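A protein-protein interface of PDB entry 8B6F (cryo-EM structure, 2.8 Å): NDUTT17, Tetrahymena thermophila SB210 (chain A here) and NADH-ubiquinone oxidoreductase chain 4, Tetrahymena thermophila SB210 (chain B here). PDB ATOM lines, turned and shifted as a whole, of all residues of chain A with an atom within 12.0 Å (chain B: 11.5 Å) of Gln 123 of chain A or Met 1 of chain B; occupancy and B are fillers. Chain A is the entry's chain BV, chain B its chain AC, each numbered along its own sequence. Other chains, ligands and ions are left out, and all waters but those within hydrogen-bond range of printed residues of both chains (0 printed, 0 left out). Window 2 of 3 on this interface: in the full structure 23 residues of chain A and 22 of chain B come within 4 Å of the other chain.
The backbone carbonyl oxygen of Ala 114 of chain A lies within hydrogen-bond range of the side-chain hydroxyl of Thr 6 of chain B, at 3.1 Å.
Hydrophobic or aromatic side chains of chain A that line the printed part of chain B: Leu 39, Ile 115, Ala 117 and Phe 120.
Of the 15 printed residues of chain B, 4 touch a printed residue of chain A.
Printed residues of chain B that touch a printed residue of chain A: Met 1, Leu 4, Thr 6 and Ile 76.
Hydrophobic or aromatic side chains of chain B within 4 Å of the printed part of chain A: Met 1, Leu 4 and Ile 76.
OD1 of Asn 3 of chain B is in hydrogen-bond range of OG1 of Thr 6 of chain B (3.2 Å).
The backbone carbonyl oxygen of Ile 76 of chain B sits at hydrogen-bond distance from the side-chain amide nitrogen of Asn 80 of chain B.
Of chain A, only Ala 117 (3.2 Å), Phe 120 (3.4 Å) and Gln 123 (3.5 Å) come within 4 Å of Met 1 of chain B.
Phe 120 of chain A touches one residue of chain B.
Gly 121 of chain A touches none of the printed residues of chain B.
No residue of chain B comes within 4 Å of Ala 124 of chain A.
No residue of chain B comes within 4 Å of Ala 125 of chain A.
No residue of chain A comes within 4 Å of Asn 3 of chain B.
Of the printed residues of chain B, Leu 39 of chain A touches Leu 4.
Of the printed residues of chain B, Ala 114 of chain A touches Thr 6.
Of the printed residues of chain B, Ile 115 of chain A touches Ile 76.
Tyr 79 of chain B touches none of the printed residues of chain A.
Asn 80 of chain B touches none of the printed residues of chain A.
The nearest residue of chain A that does not touch Met 1 of chain B is His 118 of chain A (5.2 Å).
CD1 of Leu 39 of chain A touches CD2 of Leu 4 of chain B, 3.9 Å away.
CG2 of Ile 115 of chain A touches CG1 of Ile 76 of chain B (3.9 Å).
Ala 117 of chain A touches Met 1 of chain B.
Met 1 of chain B touches Phe 120 of chain A (CE to CB, 3.4 Å).
Gln 123 of chain A touches Met 1 of chain B (NE2 to CE, 3.5 Å).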
ATOM      1  N   LEU A  39     -29.224  10.500 -14.282  1.00  0.00           N
ATOM      2  CA  LEU A  39     -28.462   9.670 -13.363  1.00  0.00           C
ATOM      3  C   LEU A  39     -27.751  10.555 -12.352  1.00  0.00           C
ATOM      4  O   LEU A  39     -27.345  11.678 -12.661  1.00  0.00           O
ATOM      5  CB  LEU A  39     -27.438   8.804 -14.111  1.00  0.00           C
ATOM      6  CG  LEU A  39     -28.023   7.820 -15.126  1.00  0.00           C
ATOM      7  CD1 LEU A  39     -26.915   7.130 -15.896  1.00  0.00           C
ATOM      8  CD2 LEU A  39     -28.907   6.791 -14.439  1.00  0.00           C
ATOM      9  N   ARG A 112     -18.825 -12.488 -17.165  1.00  0.00           N
ATOM     10  CA  ARG A 112     -20.151 -12.735 -17.720  1.00  0.00           C
ATOM     11  C   ARG A 112     -21.227 -11.978 -16.955  1.00  0.00           C
ATOM     12  O   ARG A 112     -22.231 -11.566 -17.543  1.00  0.00           O
ATOM     13  CB  ARG A 112     -20.443 -14.238 -17.711  1.00  0.00           C
ATOM     14  CG  ARG A 112     -21.854 -14.628 -18.140  1.00  0.00           C
ATOM     15  CD  ARG A 112     -22.157 -14.156 -19.550  1.00  0.00           C
ATOM     16  NE  ARG A 112     -23.368 -14.757 -20.094  1.00  0.00           N
ATOM     17  CZ  ARG A 112     -23.427 -15.958 -20.654  1.00  0.00           C
ATOM     18  NH1 ARG A 112     -22.359 -16.732 -20.746  1.00  0.00           N
ATOM     19  NH2 ARG A 112     -24.587 -16.390 -21.138  1.00  0.00           N
ATOM     20  N   ASN A 113     -21.038 -11.794 -15.650  1.00  0.00           N
ATOM     21  CA  ASN A 113     -22.055 -11.147 -14.831  1.00  0.00           C
ATOM     22  C   ASN A 113     -22.367  -9.744 -15.334  1.00  0.00           C
ATOM     23  O   ASN A 113     -23.532  -9.332 -15.368  1.00  0.00           O
ATOM     24  CB  ASN A 113     -21.588 -11.100 -13.378  1.00  0.00           C
ATOM     25  CG  ASN A 113     -22.340 -10.076 -12.558  1.00  0.00           C
ATOM     26  OD1 ASN A 113     -23.552  -9.923 -12.696  1.00  0.00           O
ATOM     27  ND2 ASN A 113     -21.619  -9.354 -11.707  1.00  0.00           N
ATOM     28  N   ALA A 114     -21.338  -8.991 -15.718  1.00  0.00           N
ATOM     29  CA  ALA A 114     -21.544  -7.609 -16.134  1.00  0.00           C
ATOM     30  C   ALA A 114     -22.390  -7.520 -17.398  1.00  0.00           C
ATOM     31  O   ALA A 114     -23.343  -6.736 -17.466  1.00  0.00           O
ATOM     32  CB  ALA A 114     -20.197  -6.929 -16.344  1.00  0.00           C
ATOM     33  N   ILE A 115     -22.053  -8.312 -18.416  1.00  0.00           N
ATOM     34  CA  ILE A 115     -22.818  -8.260 -19.658  1.00  0.00           C
ATOM     35  C   ILE A 115     -24.236  -8.776 -19.447  1.00  0.00           C
ATOM     36  O   ILE A 115     -25.181  -8.276 -20.067  1.00  0.00           O
ATOM     37  CB  ILE A 115     -22.086  -9.030 -20.774  1.00  0.00           C
ATOM     38  CG1 ILE A 115     -21.935 -10.512 -20.416  1.00  0.00           C
ATOM     39  CG2 ILE A 115     -20.726  -8.393 -21.033  1.00  0.00           C
ATOM     40  CD1 ILE A 115     -21.283 -11.345 -21.509  1.00  0.00           C
ATOM     41  N   THR A 116     -24.417  -9.770 -18.580  1.00  0.00           N
ATOM     42  CA  THR A 116     -25.746 -10.303 -18.293  1.00  0.00           C
ATOM     43  C   THR A 116     -26.425  -9.415 -17.259  1.00  0.00           C
ATOM     44  O   THR A 116     -26.052  -9.420 -16.083  1.00  0.00           O
ATOM     45  CB  THR A 116     -25.655 -11.741 -17.792  1.00  0.00           C
ATOM     46  OG1 THR A 116     -24.476 -11.903 -16.992  1.00  0.00           O
ATOM     47  CG2 THR A 116     -25.621 -12.709 -18.957  1.00  0.00           C
ATOM     48  N   ALA A 117     -27.430  -8.661 -17.696  1.00  0.00           N
ATOM     49  CA  ALA A 117     -28.168  -7.762 -16.813  1.00  0.00           C
ATOM     50  C   ALA A 117     -29.424  -8.465 -16.301  1.00  0.00           C
ATOM     51  O   ALA A 117     -30.551  -8.195 -16.719  1.00  0.00           O
ATOM     52  CB  ALA A 117     -28.501  -6.465 -17.541  1.00  0.00           C
ATOM     53  N   HIS A 118     -29.201  -9.392 -15.368  1.00  0.00           N
ATOM     54  CA  HIS A 118     -30.308 -10.121 -14.763  1.00  0.00           C
ATOM     55  C   HIS A 118     -31.051  -9.282 -13.733  1.00  0.00           C
ATOM     56  O   HIS A 118     -32.268  -9.429 -13.583  1.00  0.00           O
ATOM     57  CB  HIS A 118     -29.795 -11.403 -14.105  1.00  0.00           C
ATOM     58  CG  HIS A 118     -29.159 -12.361 -15.063  1.00  0.00           C
ATOM     59  ND1 HIS A 118     -29.472 -12.394 -16.404  1.00  0.00           N
ATOM     60  CD2 HIS A 118     -28.224 -13.321 -14.873  1.00  0.00           C
ATOM     61  CE1 HIS A 118     -28.761 -13.335 -16.998  1.00  0.00           C
ATOM     62  NE2 HIS A 118     -27.995 -13.912 -16.092  1.00  0.00           N
ATOM     63  N   ASN A 119     -30.344  -8.404 -13.020  1.00  0.00           N
ATOM     64  CA  ASN A 119     -30.941  -7.622 -11.937  1.00  0.00           C
ATOM     65  C   ASN A 119     -31.667  -6.411 -12.523  1.00  0.00           C
ATOM     66  O   ASN A 119     -31.291  -5.252 -12.333  1.00  0.00           O
ATOM     67  CB  ASN A 119     -29.874  -7.206 -10.937  1.00  0.00           C
ATOM     68  CG  ASN A 119     -29.159  -8.393 -10.325  1.00  0.00           C
ATOM     69  OD1 ASN A 119     -29.622  -8.970  -9.341  1.00  0.00           O
ATOM     70  ND2 ASN A 119     -28.024  -8.763 -10.906  1.00  0.00           N
ATOM     71  N   PHE A 120     -32.736  -6.707 -13.255  1.00  0.00           N
ATOM     72  CA  PHE A 120     -33.627  -5.701 -13.814  1.00  0.00           C
ATOM     73  C   PHE A 120     -35.000  -5.902 -13.193  1.00  0.00           C
ATOM     74  O   PHE A 120     -35.504  -7.027 -13.152  1.00  0.00           O
ATOM     75  CB  PHE A 120     -33.689  -5.814 -15.338  1.00  0.00           C
ATOM     76  CG  PHE A 120     -34.223  -4.588 -16.018  1.00  0.00           C
ATOM     77  CD1 PHE A 120     -33.385  -3.531 -16.328  1.00  0.00           C
ATOM     78  CD2 PHE A 120     -35.558  -4.500 -16.364  1.00  0.00           C
ATOM     79  CE1 PHE A 120     -33.873  -2.407 -16.958  1.00  0.00           C
ATOM     80  CE2 PHE A 120     -36.050  -3.380 -16.993  1.00  0.00           C
ATOM     81  CZ  PHE A 120     -35.208  -2.333 -17.290  1.00  0.00           C
ATOM     82  N   GLY A 121     -35.601  -4.819 -12.706  1.00  0.00           N
ATOM     83  CA  GLY A 121     -36.811  -4.948 -11.912  1.00  0.00           C
ATOM     84  C   GLY A 121     -38.061  -5.268 -12.702  1.00  0.00           C
ATOM     85  O   GLY A 121     -39.107  -5.515 -12.091  1.00  0.00           O
ATOM     86  N   TRP A 122     -37.984  -5.282 -14.030  1.00  0.00           N
ATOM     87  CA  TRP A 122     -39.162  -5.483 -14.863  1.00  0.00           C
ATOM     88  C   TRP A 122     -39.533  -6.949 -15.032  1.00  0.00           C
ATOM     89  O   TRP A 122     -40.527  -7.246 -15.701  1.00  0.00           O
ATOM     90  CB  TRP A 122     -38.941  -4.842 -16.236  1.00  0.00           C
ATOM     91  CG  TRP A 122     -40.162  -4.833 -17.099  1.00  0.00           C
ATOM     92  CD1 TRP A 122     -40.400  -5.616 -18.189  1.00  0.00           C
ATOM     93  CD2 TRP A 122     -41.318  -4.006 -16.939  1.00  0.00           C
ATOM     94  NE1 TRP A 122     -41.633  -5.324 -18.720  1.00  0.00           N
ATOM     95  CE2 TRP A 122     -42.216  -4.337 -17.971  1.00  0.00           C
ATOM     96  CE3 TRP A 122     -41.679  -3.014 -16.023  1.00  0.00           C
ATOM     97  CZ2 TRP A 122     -43.452  -3.715 -18.114  1.00  0.00           C
ATOM     98  CZ3 TRP A 122     -42.907  -2.395 -16.167  1.00  0.00           C
ATOM     99  CH2 TRP A 122     -43.779  -2.747 -17.205  1.00  0.00           C
ATOM    100  N   GLN A 123     -38.771  -7.874 -14.449  1.00  0.00           N
ATOM    101  CA  GLN A 123     -39.109  -9.287 -14.554  1.00  0.00           C
ATOM    102  C   GLN A 123     -40.506  -9.518 -13.995  1.00  0.00           C
ATOM    103  O   GLN A 123     -40.734  -9.355 -12.794  1.00  0.00           O
ATOM    104  CB  GLN A 123     -38.092 -10.153 -13.807  1.00  0.00           C
ATOM    105  CG  GLN A 123     -36.638  -9.863 -14.140  1.00  0.00           C
ATOM    106  CD  GLN A 123     -36.333  -9.964 -15.618  1.00  0.00           C
ATOM    107  OE1 GLN A 123     -37.095 -10.552 -16.382  1.00  0.00           O
ATOM    108  NE2 GLN A 123     -35.211  -9.386 -16.030  1.00  0.00           N
ATOM    109  N   ALA A 124     -41.447  -9.883 -14.858  1.00  0.00           N
ATOM    110  CA  ALA A 124     -42.827 -10.109 -14.454  1.00  0.00           C
ATOM    111  C   ALA A 124     -43.510 -10.929 -15.542  1.00  0.00           C
ATOM    112  O   ALA A 124     -42.857 -11.446 -16.454  1.00  0.00           O
ATOM    113  CB  ALA A 124     -43.543  -8.779 -14.196  1.00  0.00           C
ATOM    114  N   ALA A 125     -44.828 -11.056 -15.441  1.00  0.00           N
ATOM    115  CA  ALA A 125     -45.611 -11.785 -16.431  1.00  0.00           C
ATOM    116  C   ALA A 125     -45.178 -13.245 -16.492  1.00  0.00           C
ATOM    117  O   ALA A 125     -45.511 -14.038 -15.611  1.00  0.00           O
ATOM    118  CB  ALA A 125     -45.477 -11.132 -17.800  1.00  0.00           C
ATOM    119  N   MET B   1     -32.123  -3.152 -21.405  1.00  0.00           N
ATOM    120  CA  MET B   1     -31.618  -3.664 -20.099  1.00  0.00           C
ATOM    121  C   MET B   1     -30.168  -3.257 -19.868  1.00  0.00           C
ATOM    122  O   MET B   1     -29.605  -3.511 -18.805  1.00  0.00           O
ATOM    123  CB  MET B   1     -31.749  -5.185 -20.033  1.00  0.00           C
ATOM    124  CG  MET B   1     -33.146  -5.690 -20.356  1.00  0.00           C
ATOM    125  SD  MET B   1     -33.354  -7.447 -20.027  1.00  0.00           S
ATOM    126  CE  MET B   1     -33.256  -7.457 -18.240  1.00  0.00           C
ATOM    127  N   PHE B   2     -29.565  -2.628 -20.874  1.00  0.00           N
ATOM    128  CA  PHE B   2     -28.205  -2.128 -20.735  1.00  0.00           C
ATOM    129  C   PHE B   2     -28.159  -1.064 -19.647  1.00  0.00           C
ATOM    130  O   PHE B   2     -29.035  -0.200 -19.561  1.00  0.00           O
ATOM    131  CB  PHE B   2     -27.725  -1.560 -22.069  1.00  0.00           C
ATOM    132  CG  PHE B   2     -26.274  -1.193 -22.091  1.00  0.00           C
ATOM    133  CD1 PHE B   2     -25.299  -2.174 -22.109  1.00  0.00           C
ATOM    134  CD2 PHE B   2     -25.883   0.133 -22.119  1.00  0.00           C
ATOM    135  CE1 PHE B   2     -23.964  -1.840 -22.142  1.00  0.00           C
ATOM    136  CE2 PHE B   2     -24.548   0.473 -22.152  1.00  0.00           C
ATOM    137  CZ  PHE B   2     -23.588  -0.515 -22.164  1.00  0.00           C
ATOM    138  N   ASN B   3     -27.126  -1.127 -18.809  1.00  0.00           N
ATOM    139  CA  ASN B   3     -27.002  -0.247 -17.659  1.00  0.00           C
ATOM    140  C   ASN B   3     -25.614   0.374 -17.617  1.00  0.00           C
ATOM    141  O   ASN B   3     -24.681  -0.072 -18.291  1.00  0.00           O
ATOM    142  CB  ASN B   3     -27.280  -0.991 -16.347  1.00  0.00           C
ATOM    143  CG  ASN B   3     -26.544  -2.309 -16.258  1.00  0.00           C
ATOM    144  OD1 ASN B   3     -25.647  -2.585 -17.052  1.00  0.00           O
ATOM    145  ND2 ASN B   3     -26.920  -3.132 -15.287  1.00  0.00           N
ATOM    146  N   LEU B   4     -25.496   1.421 -16.801  1.00  0.00           N
ATOM    147  CA  LEU B   4     -24.247   2.161 -16.680  1.00  0.00           C
ATOM    148  C   LEU B   4     -23.113   1.301 -16.138  1.00  0.00           C
ATOM    149  O   LEU B   4     -21.943   1.626 -16.363  1.00  0.00           O
ATOM    150  CB  LEU B   4     -24.467   3.377 -15.781  1.00  0.00           C
ATOM    151  CG  LEU B   4     -23.270   4.287 -15.523  1.00  0.00           C
ATOM    152  CD1 LEU B   4     -22.743   4.875 -16.821  1.00  0.00           C
ATOM    153  CD2 LEU B   4     -23.657   5.386 -14.558  1.00  0.00           C
ATOM    154  N   ASN B   5     -23.429   0.213 -15.435  1.00  0.00           N
ATOM    155  CA  ASN B   5     -22.381  -0.654 -14.906  1.00  0.00           C
ATOM    156  C   ASN B   5     -21.534  -1.238 -16.027  1.00  0.00           C
ATOM    157  O   ASN B   5     -20.304  -1.294 -15.921  1.00  0.00           O
ATOM    158  CB  ASN B   5     -22.997  -1.771 -14.065  1.00  0.00           C
ATOM    159  CG  ASN B   5     -23.576  -1.266 -12.761  1.00  0.00           C
ATOM    160  OD1 ASN B   5     -23.136  -0.251 -12.225  1.00  0.00           O
ATOM    161  ND2 ASN B   5     -24.569  -1.977 -12.241  1.00  0.00           N
ATOM    162  N   THR B   6     -22.172  -1.683 -17.110  1.00  0.00           N
ATOM    163  CA  THR B   6     -21.421  -2.232 -18.234  1.00  0.00           C
ATOM    164  C   THR B   6     -20.547  -1.163 -18.878  1.00  0.00           C
ATOM    165  O   THR B   6     -19.407  -1.436 -19.269  1.00  0.00           O
ATOM    166  CB  THR B   6     -22.373  -2.838 -19.263  1.00  0.00           C
ATOM    167  OG1 THR B   6     -23.209  -3.814 -18.632  1.00  0.00           O
ATOM    168  CG2 THR B   6     -21.590  -3.506 -20.388  1.00  0.00           C
ATOM    169  N   ILE B   7     -21.072   0.056 -19.018  1.00  0.00           N
ATOM    170  CA  ILE B   7     -20.282   1.139 -19.597  1.00  0.00           C
ATOM    171  C   ILE B   7     -19.018   1.368 -18.783  1.00  0.00           C
ATOM    172  O   ILE B   7     -17.908   1.416 -19.324  1.00  0.00           O
ATOM    173  CB  ILE B   7     -21.121   2.427 -19.681  1.00  0.00           C
ATOM    174  CG1 ILE B   7     -22.378   2.199 -20.521  1.00  0.00           C
ATOM    175  CG2 ILE B   7     -20.271   3.581 -20.190  1.00  0.00           C
ATOM    176  CD1 ILE B   7     -23.330   3.372 -20.528  1.00  0.00           C
ATOM    177  N   ILE B  76     -20.389  -5.041 -26.452  1.00  0.00           N
ATOM    178  CA  ILE B  76     -21.697  -4.798 -25.854  1.00  0.00           C
ATOM    179  C   ILE B  76     -21.944  -3.299 -25.744  1.00  0.00           C
ATOM    180  O   ILE B  76     -23.032  -2.806 -26.060  1.00  0.00           O
ATOM    181  CB  ILE B  76     -21.794  -5.495 -24.484  1.00  0.00           C
ATOM    182  CG1 ILE B  76     -21.455  -6.985 -24.603  1.00  0.00           C
ATOM    183  CG2 ILE B  76     -23.178  -5.313 -23.889  1.00  0.00           C
ATOM    184  CD1 ILE B  76     -22.267  -7.736 -25.627  1.00  0.00           C
ATOM    185  N   TYR B  77     -20.934  -2.553 -25.291  1.00  0.00           N
ATOM    186  CA  TYR B  77     -21.096  -1.118 -25.077  1.00  0.00           C
ATOM    187  C   TYR B  77     -21.419  -0.396 -26.379  1.00  0.00           C
ATOM    188  O   TYR B  77     -22.323   0.445 -26.430  1.00  0.00           O
ATOM    189  CB  TYR B  77     -19.822  -0.549 -24.447  1.00  0.00           C
ATOM    190  CG  TYR B  77     -19.867   0.932 -24.130  1.00  0.00           C
ATOM    191  CD1 TYR B  77     -21.070   1.628 -24.090  1.00  0.00           C
ATOM    192  CD2 TYR B  77     -18.697   1.636 -23.878  1.00  0.00           C
ATOM    193  CE1 TYR B  77     -21.105   2.974 -23.806  1.00  0.00           C
ATOM    194  CE2 TYR B  77     -18.723   2.983 -23.595  1.00  0.00           C
ATOM    195  CZ  TYR B  77     -19.930   3.646 -23.564  1.00  0.00           C
ATOM    196  OH  TYR B  77     -19.960   4.987 -23.276  1.00  0.00           O
ATOM    197  N   TYR B  79     -22.654  -1.668 -29.239  1.00  0.00           N
ATOM    198  CA  TYR B  79     -23.963  -2.072 -29.735  1.00  0.00           C
ATOM    199  C   TYR B  79     -25.077  -1.337 -29.002  1.00  0.00           C
ATOM    200  O   TYR B  79     -26.010  -0.818 -29.626  1.00  0.00           O
ATOM    201  CB  TYR B  79     -24.123  -3.585 -29.585  1.00  0.00           C
ATOM    202  CG  TYR B  79     -25.451  -4.118 -30.062  1.00  0.00           C
ATOM    203  CD1 TYR B  79     -25.744  -4.204 -31.414  1.00  0.00           C
ATOM    204  CD2 TYR B  79     -26.404  -4.558 -29.155  1.00  0.00           C
ATOM    205  CE1 TYR B  79     -26.956  -4.697 -31.849  1.00  0.00           C
ATOM    206  CE2 TYR B  79     -27.617  -5.053 -29.579  1.00  0.00           C
ATOM    207  CZ  TYR B  79     -27.888  -5.121 -30.927  1.00  0.00           C
ATOM    208  OH  TYR B  79     -29.097  -5.617 -31.354  1.00  0.00           O
ATOM    209  N   ASN B  80     -24.995  -1.277 -27.672  1.00  0.00           N
ATOM    210  CA  ASN B  80     -26.057  -0.643 -26.899  1.00  0.00           C
ATOM    211  C   ASN B  80     -26.031   0.873 -27.039  1.00  0.00           C
ATOM    212  O   ASN B  80     -27.077   1.521 -26.927  1.00  0.00           O
ATOM    213  CB  ASN B  80     -25.953  -1.051 -25.433  1.00  0.00           C
ATOM    214  CG  ASN B  80     -26.298  -2.507 -25.216  1.00  0.00           C
ATOM    215  OD1 ASN B  80     -27.469  -2.873 -25.131  1.00  0.00           O
ATOM    216  ND2 ASN B  80     -25.279  -3.348 -25.123  1.00  0.00           N
ATOM    217  N   LEU B  81     -24.856   1.457 -27.277  1.00  0.00           N
ATOM    218  CA  LEU B  81     -24.791   2.890 -27.544  1.00  0.00           C
ATOM    219  C   LEU B  81     -25.480   3.225 -28.858  1.00  0.00           C
ATOM    220  O   LEU B  81     -26.241   4.195 -28.937  1.00  0.00           O
ATOM    221  CB  LEU B  81     -23.333   3.357 -27.556  1.00  0.00           C
ATOM    222  CG  LEU B  81     -23.036   4.864 -27.582  1.00  0.00           C
ATOM    223  CD1 LEU B  81     -21.586   5.110 -27.216  1.00  0.00           C
ATOM    224  CD2 LEU B  81     -23.327   5.515 -28.930  1.00  0.00           C
ATOM    225  N   LEU B  83     -27.855   1.462 -30.190  1.00  0.00           N
ATOM    226  CA  LEU B  83     -29.276   1.272 -29.924  1.00  0.00           C
ATOM    227  C   LEU B  83     -29.866   2.465 -29.184  1.00  0.00           C
ATOM    228  O   LEU B  83     -30.976   2.910 -29.497  1.00  0.00           O
ATOM    229  CB  LEU B  83     -29.503  -0.009 -29.121  1.00  0.00           C
ATOM    230  CG  LEU B  83     -29.295  -1.347 -29.835  1.00  0.00           C
ATOM    231  CD1 LEU B  83     -29.747  -2.482 -28.933  1.00  0.00           C
ATOM    232  CD2 LEU B  83     -30.006  -1.411 -31.178  1.00  0.00           C
ATOM    233  N   ASN B  84     -29.142   2.998 -28.200  1.00  0.00           N
ATOM    234  CA  ASN B  84     -29.657   4.145 -27.459  1.00  0.00           C
ATOM    235  C   ASN B  84     -29.839   5.352 -28.369  1.00  0.00           C
ATOM    236  O   ASN B  84     -30.842   6.066 -28.269  1.00  0.00           O
ATOM    237  CB  ASN B  84     -28.714   4.491 -26.306  1.00  0.00           C
ATOM    238  CG  ASN B  84     -28.647   3.399 -25.261  1.00  0.00           C
ATOM    239  OD1 ASN B  84     -29.596   2.638 -25.077  1.00  0.00           O
ATOM    240  ND2 ASN B  84     -27.521   3.318 -24.563  1.00  0.00           N
ATOM    241  N   SER B  87     -32.818   4.335 -31.105  1.00  0.00           N
ATOM    242  CA  SER B  87     -34.154   3.902 -30.709  1.00  0.00           C
ATOM    243  C   SER B  87     -35.090   5.086 -30.497  1.00  0.00           C
ATOM    244  O   SER B  87     -36.200   5.115 -31.040  1.00  0.00           O
ATOM    245  CB  SER B  87     -34.072   3.052 -29.440  1.00  0.00           C
ATOM    246  OG  SER B  87     -33.524   3.792 -28.363  1.00  0.00           O
